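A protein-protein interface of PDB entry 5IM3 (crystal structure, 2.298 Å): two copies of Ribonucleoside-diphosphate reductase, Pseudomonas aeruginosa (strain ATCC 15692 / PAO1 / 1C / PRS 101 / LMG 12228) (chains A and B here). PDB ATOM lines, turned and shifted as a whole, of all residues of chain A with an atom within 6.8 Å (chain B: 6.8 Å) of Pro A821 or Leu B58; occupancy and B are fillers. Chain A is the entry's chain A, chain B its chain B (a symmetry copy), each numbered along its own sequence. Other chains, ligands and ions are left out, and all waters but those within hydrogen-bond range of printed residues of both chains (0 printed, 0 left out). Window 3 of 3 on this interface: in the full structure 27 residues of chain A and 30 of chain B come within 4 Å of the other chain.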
ATOM      1  N   ARG A 215      30.288  17.724  -0.424  1.00  0.00           N
ATOM      2  CA  ARG A 215      29.332  17.113   0.491  1.00  0.00           C
ATOM      3  C   ARG A 215      29.666  17.361   1.956  1.00  0.00           C
ATOM      4  O   ARG A 215      28.799  17.164   2.814  1.00  0.00           O
ATOM      5  CB  ARG A 215      29.253  15.602   0.243  1.00  0.00           C
ATOM      6  CG  ARG A 215      28.788  15.219  -1.160  1.00  0.00           C
ATOM      7  CD  ARG A 215      27.333  15.614  -1.433  1.00  0.00           C
ATOM      8  NE  ARG A 215      26.364  14.721  -0.790  1.00  0.00           N
ATOM      9  CZ  ARG A 215      25.608  15.036   0.261  1.00  0.00           C
ATOM     10  NH1 ARG A 215      25.684  16.236   0.825  1.00  0.00           N
ATOM     11  NH2 ARG A 215      24.761  14.141   0.753  1.00  0.00           N
ATOM     12  N   TRP A 819      20.320  18.633   4.543  1.00  0.00           N
ATOM     13  CA  TRP A 819      21.541  18.496   3.753  1.00  0.00           C
ATOM     14  C   TRP A 819      21.562  17.102   3.138  1.00  0.00           C
ATOM     15  O   TRP A 819      21.798  16.108   3.835  1.00  0.00           O
ATOM     16  CB  TRP A 819      22.779  18.744   4.613  1.00  0.00           C
ATOM     17  CG  TRP A 819      24.063  18.737   3.827  1.00  0.00           C
ATOM     18  CD1 TRP A 819      25.103  17.865   3.967  1.00  0.00           C
ATOM     19  CD2 TRP A 819      24.437  19.639   2.773  1.00  0.00           C
ATOM     20  NE1 TRP A 819      26.102  18.169   3.073  1.00  0.00           N
ATOM     21  CE2 TRP A 819      25.718  19.253   2.329  1.00  0.00           C
ATOM     22  CE3 TRP A 819      23.815  20.736   2.167  1.00  0.00           C
ATOM     23  CZ2 TRP A 819      26.388  19.925   1.307  1.00  0.00           C
ATOM     24  CZ3 TRP A 819      24.486  21.402   1.150  1.00  0.00           C
ATOM     25  CH2 TRP A 819      25.757  20.993   0.732  1.00  0.00           C
ATOM     26  N   ASP A 820      21.314  17.031   1.835  1.00  0.00           N
ATOM     27  CA  ASP A 820      21.216  15.762   1.127  1.00  0.00           C
ATOM     28  C   ASP A 820      21.494  16.021  -0.347  1.00  0.00           C
ATOM     29  O   ASP A 820      21.608  17.180  -0.771  1.00  0.00           O
ATOM     30  CB  ASP A 820      19.834  15.113   1.329  1.00  0.00           C
ATOM     31  CG  ASP A 820      18.698  16.111   1.245  1.00  0.00           C
ATOM     32  OD1 ASP A 820      18.697  16.944   0.316  1.00  0.00           O
ATOM     33  OD2 ASP A 820      17.802  16.056   2.111  1.00  0.00           O
ATOM     34  N   PRO A 821      21.633  14.964  -1.154  1.00  0.00           N
ATOM     35  CA  PRO A 821      21.951  15.171  -2.578  1.00  0.00           C
ATOM     36  C   PRO A 821      20.993  16.092  -3.320  1.00  0.00           C
ATOM     37  O   PRO A 821      21.454  16.906  -4.131  1.00  0.00           O
ATOM     38  CB  PRO A 821      21.918  13.745  -3.138  1.00  0.00           C
ATOM     39  CG  PRO A 821      22.355  12.903  -1.998  1.00  0.00           C
ATOM     40  CD  PRO A 821      21.787  13.552  -0.762  1.00  0.00           C
ATOM     41  N   VAL A 822      19.682  15.998  -3.082  1.00  0.00           N
ATOM     42  CA  VAL A 822      18.752  16.843  -3.829  1.00  0.00           C
ATOM     43  C   VAL A 822      18.975  18.311  -3.486  1.00  0.00           C
ATOM     44  O   VAL A 822      18.904  19.182  -4.360  1.00  0.00           O
ATOM     45  CB  VAL A 822      17.293  16.414  -3.576  1.00  0.00           C
ATOM     46  CG1 VAL A 822      17.066  14.980  -4.040  1.00  0.00           C
ATOM     47  CG2 VAL A 822      16.926  16.566  -2.114  1.00  0.00           C
ATOM     48  N   MET A 823      19.257  18.611  -2.215  1.00  0.00           N
ATOM     49  CA  MET A 823      19.556  19.986  -1.830  1.00  0.00           C
ATOM     50  C   MET A 823      20.782  20.503  -2.569  1.00  0.00           C
ATOM     51  O   MET A 823      20.808  21.654  -3.017  1.00  0.00           O
ATOM     52  CB  MET A 823      19.764  20.074  -0.318  1.00  0.00           C
ATOM     53  CG  MET A 823      20.139  21.463   0.187  1.00  0.00           C
ATOM     54  SD  MET A 823      18.887  22.718  -0.154  1.00  0.00           S
ATOM     55  CE  MET A 823      17.511  22.112   0.824  1.00  0.00           C
ATOM     56  N   VAL A 824      21.811  19.663  -2.707  1.00  0.00           N
ATOM     57  CA  VAL A 824      23.004  20.063  -3.448  1.00  0.00           C
ATOM     58  C   VAL A 824      22.657  20.342  -4.903  1.00  0.00           C
ATOM     59  O   VAL A 824      23.131  21.319  -5.493  1.00  0.00           O
ATOM     60  CB  VAL A 824      24.094  18.980  -3.325  1.00  0.00           C
ATOM     61  CG1 VAL A 824      25.279  19.292  -4.236  1.00  0.00           C
ATOM     62  CG2 VAL A 824      24.547  18.853  -1.879  1.00  0.00           C
ATOM     63  N   ASN A 825      21.836  19.480  -5.509  1.00  0.00           N
ATOM     64  CA  ASN A 825      21.452  19.676  -6.901  1.00  0.00           C
ATOM     65  C   ASN A 825      20.608  20.930  -7.080  1.00  0.00           C
ATOM     66  O   ASN A 825      20.650  21.557  -8.145  1.00  0.00           O
ATOM     67  CB  ASN A 825      20.695  18.450  -7.411  1.00  0.00           C
ATOM     68  CG  ASN A 825      20.382  18.533  -8.890  1.00  0.00           C
ATOM     69  OD1 ASN A 825      21.246  18.293  -9.733  1.00  0.00           O
ATOM     70  ND2 ASN A 825      19.136  18.864  -9.216  1.00  0.00           N
ATOM     71  N   ASP A 826      19.840  21.314  -6.057  1.00  0.00           N
ATOM     72  CA  ASP A 826      19.051  22.538  -6.146  1.00  0.00           C
ATOM     73  C   ASP A 826      19.935  23.772  -6.018  1.00  0.00           C
ATOM     74  O   ASP A 826      19.714  24.773  -6.708  1.00  0.00           O
ATOM     75  CB  ASP A 826      17.963  22.549  -5.069  1.00  0.00           C
ATOM     76  CG  ASP A 826      16.778  21.669  -5.424  1.00  0.00           C
ATOM     77  OD1 ASP A 826      16.582  21.383  -6.624  1.00  0.00           O
ATOM     78  OD2 ASP A 826      16.035  21.266  -4.502  1.00  0.00           O
ATOM     79  N   ARG A 839      11.973  23.812   0.535  1.00  0.00           N
ATOM     80  CA  ARG A 839      12.295  23.031   1.724  1.00  0.00           C
ATOM     81  C   ARG A 839      13.046  23.828   2.785  1.00  0.00           C
ATOM     82  O   ARG A 839      13.023  23.441   3.957  1.00  0.00           O
ATOM     83  CB  ARG A 839      13.107  21.801   1.331  1.00  0.00           C
ATOM     84  CG  ARG A 839      12.283  20.731   0.631  1.00  0.00           C
ATOM     85  CD  ARG A 839      13.178  19.662   0.051  1.00  0.00           C
ATOM     86  NE  ARG A 839      13.945  18.982   1.093  1.00  0.00           N
ATOM     87  CZ  ARG A 839      15.218  18.613   0.979  1.00  0.00           C
ATOM     88  NH1 ARG A 839      15.902  18.864  -0.130  1.00  0.00           N
ATOM     89  NH2 ARG A 839      15.817  18.000   1.991  1.00  0.00           N
ATOM     90  N   ILE B  53      11.351  11.916  -6.994  1.00  0.00           N
ATOM     91  CA  ILE B  53      11.805  11.699  -8.365  1.00  0.00           C
ATOM     92  C   ILE B  53      13.250  12.151  -8.523  1.00  0.00           C
ATOM     93  O   ILE B  53      14.033  11.531  -9.253  1.00  0.00           O
ATOM     94  CB  ILE B  53      10.874  12.422  -9.357  1.00  0.00           C
ATOM     95  CG1 ILE B  53       9.460  11.844  -9.259  1.00  0.00           C
ATOM     96  CG2 ILE B  53      11.401  12.296 -10.783  1.00  0.00           C
ATOM     97  CD1 ILE B  53       8.452  12.543 -10.143  1.00  0.00           C
ATOM     98  N   THR B  54      13.629  13.235  -7.840  1.00  0.00           N
ATOM     99  CA  THR B  54      14.990  13.744  -7.966  1.00  0.00           C
ATOM    100  C   THR B  54      16.002  12.757  -7.394  1.00  0.00           C
ATOM    101  O   THR B  54      17.069  12.549  -7.982  1.00  0.00           O
ATOM    102  CB  THR B  54      15.114  15.103  -7.275  1.00  0.00           C
ATOM    103  OG1 THR B  54      14.102  15.986  -7.773  1.00  0.00           O
ATOM    104  CG2 THR B  54      16.484  15.722  -7.537  1.00  0.00           C
ATOM    105  N   LYS B  55      15.689  12.141  -6.250  1.00  0.00           N
ATOM    106  CA  LYS B  55      16.603  11.153  -5.684  1.00  0.00           C
ATOM    107  C   LYS B  55      16.879  10.035  -6.679  1.00  0.00           C
ATOM    108  O   LYS B  55      18.004   9.531  -6.763  1.00  0.00           O
ATOM    109  CB  LYS B  55      16.032  10.574  -4.389  1.00  0.00           C
ATOM    110  CG  LYS B  55      15.936  11.558  -3.234  1.00  0.00           C
ATOM    111  CD  LYS B  55      15.472  10.846  -1.975  1.00  0.00           C
ATOM    112  CE  LYS B  55      15.129  11.815  -0.858  1.00  0.00           C
ATOM    113  NZ  LYS B  55      14.562  11.103   0.325  1.00  0.00           N
ATOM    114  N   ALA B  56      15.867   9.642  -7.454  1.00  0.00           N
ATOM    115  CA  ALA B  56      16.060   8.572  -8.426  1.00  0.00           C
ATOM    116  C   ALA B  56      16.936   9.035  -9.585  1.00  0.00           C
ATOM    117  O   ALA B  56      17.801   8.285 -10.052  1.00  0.00           O
ATOM    118  CB  ALA B  56      14.706   8.071  -8.929  1.00  0.00           C
ATOM    119  N   PHE B  57      16.732  10.266 -10.062  1.00  0.00           N
ATOM    120  CA  PHE B  57      17.626  10.818 -11.076  1.00  0.00           C
ATOM    121  C   PHE B  57      19.062  10.881 -10.569  1.00  0.00           C
ATOM    122  O   PHE B  57      19.997  10.513 -11.289  1.00  0.00           O
ATOM    123  CB  PHE B  57      17.152  12.208 -11.504  1.00  0.00           C
ATOM    124  CG  PHE B  57      16.177  12.190 -12.649  1.00  0.00           C
ATOM    125  CD1 PHE B  57      16.626  12.187 -13.959  1.00  0.00           C
ATOM    126  CD2 PHE B  57      14.811  12.177 -12.416  1.00  0.00           C
ATOM    127  CE1 PHE B  57      15.733  12.171 -15.015  1.00  0.00           C
ATOM    128  CE2 PHE B  57      13.914  12.162 -13.467  1.00  0.00           C
ATOM    129  CZ  PHE B  57      14.374  12.157 -14.766  1.00  0.00           C
ATOM    130  N   LEU B  58      19.259  11.342  -9.329  1.00  0.00           N
ATOM    131  CA  LEU B  58      20.610  11.454  -8.790  1.00  0.00           C
ATOM    132  C   LEU B  58      21.239  10.089  -8.550  1.00  0.00           C
ATOM    133  O   LEU B  58      22.468   9.968  -8.562  1.00  0.00           O
ATOM    134  CB  LEU B  58      20.599  12.258  -7.488  1.00  0.00           C
ATOM    135  CG  LEU B  58      20.187  13.727  -7.590  1.00  0.00           C
ATOM    136  CD1 LEU B  58      20.116  14.350  -6.206  1.00  0.00           C
ATOM    137  CD2 LEU B  58      21.149  14.505  -8.475  1.00  0.00           C
ATOM    138  N   ALA B  59      20.427   9.056  -8.321  1.00  0.00           N
ATOM    139  CA  ALA B  59      20.975   7.720  -8.136  1.00  0.00           C
ATOM    140  C   ALA B  59      21.601   7.177  -9.414  1.00  0.00           C
ATOM    141  O   ALA B  59      22.466   6.298  -9.341  1.00  0.00           O
ATOM    142  CB  ALA B  59      19.886   6.769  -7.641  1.00  0.00           C
ATOM    143  N   VAL B  60      21.188   7.683 -10.576  1.00  0.00           N
ATOM    144  CA  VAL B  60      21.746   7.217 -11.842  1.00  0.00           C
ATOM    145  C   VAL B  60      23.064   7.922 -12.138  1.00  0.00           C
ATOM    146  O   VAL B  60      24.125   7.289 -12.200  1.00  0.00           O
ATOM    147  CB  VAL B  60      20.729   7.421 -12.981  1.00  0.00           C
ATOM    148  CG1 VAL B  60      21.281   6.887 -14.296  1.00  0.00           C
ATOM    149  CG2 VAL B  60      19.411   6.740 -12.644  1.00  0.00           C
ATOM    150  N   GLU B  61      23.015   9.237 -12.328  1.00  0.00           N
ATOM    151  CA  GLU B  61      24.226  10.022 -12.565  1.00  0.00           C
ATOM    152  C   GLU B  61      24.673  10.723 -11.282  1.00  0.00           C
ATOM    153  O   GLU B  61      24.454  11.921 -11.104  1.00  0.00           O
ATOM    154  CB  GLU B  61      24.006  11.052 -13.681  1.00  0.00           C
ATOM    155  CG  GLU B  61      22.717  11.863 -13.571  1.00  0.00           C
ATOM    156  CD  GLU B  61      21.590  11.298 -14.415  1.00  0.00           C
ATOM    157  OE1 GLU B  61      21.705  10.141 -14.875  1.00  0.00           O
ATOM    158  OE2 GLU B  61      20.587  12.013 -14.626  1.00  0.00           O
ATOM    159  N   SER B  68      24.011  16.405 -15.076  1.00  0.00           N
ATOM    160  CA  SER B  68      23.018  16.474 -14.010  1.00  0.00           C
ATOM    161  C   SER B  68      22.331  17.830 -13.940  1.00  0.00           C
ATOM    162  O   SER B  68      21.422  18.003 -13.119  1.00  0.00           O
ATOM    163  CB  SER B  68      23.680  16.168 -12.664  1.00  0.00           C
ATOM    164  OG  SER B  68      24.424  14.963 -12.718  1.00  0.00           O
ATOM    165  N   ILE B  71      18.466  17.922 -14.585  1.00  0.00           N
ATOM    166  CA  ILE B  71      17.574  17.162 -13.713  1.00  0.00           C
ATOM    167  C   ILE B  71      16.444  18.047 -13.203  1.00  0.00           C
ATOM    168  O   ILE B  71      15.264  17.683 -13.277  1.00  0.00           O
ATOM    169  CB  ILE B  71      18.365  16.535 -12.551  1.00  0.00           C
ATOM    170  CG1 ILE B  71      19.305  15.450 -13.082  1.00  0.00           C
ATOM    171  CG2 ILE B  71      17.412  15.957 -11.493  1.00  0.00           C
ATOM    172  CD1 ILE B  71      20.189  14.830 -12.024  1.00  0.00           C
ATOM    173  N   VAL B 117      15.908   5.663 -14.884  1.00  0.00           N
ATOM    174  CA  VAL B 117      15.383   6.222 -13.644  1.00  0.00           C
ATOM    175  C   VAL B 117      14.143   5.459 -13.197  1.00  0.00           C
ATOM    176  O   VAL B 117      13.944   5.221 -12.000  1.00  0.00           O
ATOM    177  CB  VAL B 117      15.093   7.724 -13.829  1.00  0.00           C
ATOM    178  CG1 VAL B 117      14.483   8.319 -12.569  1.00  0.00           C
ATOM    179  CG2 VAL B 117      16.369   8.459 -14.196  1.00  0.00           C
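The side-chain amide oxygen of Asn A825 sits close to the backbone carbonyl oxygen of Ser B68 (3.4 Å).
The backbone carbonyl oxygen (O) of Glu B61 lies within hydrogen-bond range of the side-chain hydroxyl (OG) of Ser B68.
Pro A821 touches Leu B58. CG2 of Thr B54 touches CG1 of Val A822, at 3.6 Å. Val A822 touches Lys B55 (CG1 to CG, 3.7 Å). Leu B58 touches Val A822 (CD1 to N, 3.6 Å). Asn A825 touches Leu B58.
Pro A821 touches just one residue of chain B: Leu B58. Of the printed residues of chain B, Val A822 touches Thr B54 (3.6 Å), Lys B55 (3.7 Å) and Leu B58 (3.6 Å). Printed residues of chain B within 4 Å of Asn A825: Leu B58 (3.99 Å) and Ser B68 (3.4 Å). Of the printed residues of chain A, Lys B55 touches Val A822. Printed residues of chain A within 4 Å of Leu B58: Pro A821 (3.5 Å), Val A822 (3.6 Å) and Asn A825 (3.99 Å). Val B60 touches none of the printed residues of chain A. Printed residues of chain A within 4 Å of Ser B68: Asn A825. The nearest printed residue of chain A that does not touch Leu B58 is Met A823 (5.9 Å).
Of the 12 printed residues of chain B, 4 touch a printed residue of chain A. Printed residues of chain B that touch a printed residue of chain A: Thr B54, Lys B55, Leu B58 and Ser B68. Hydrophobic or aromatic side chains of chain B that line the printed part of chain A: Leu B58. Of the 10 printed residues of chain A, 3 touch a printed residue of chain B. Hydrophobic or aromatic side chains of chain A within 4 Å of the printed part of chain B: Pro A821 and Val A822.
No position is printed for both chains. Of the 6 pairs that touch across the chains among the printed residues, none has its exchanged pair printed and touching as well.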
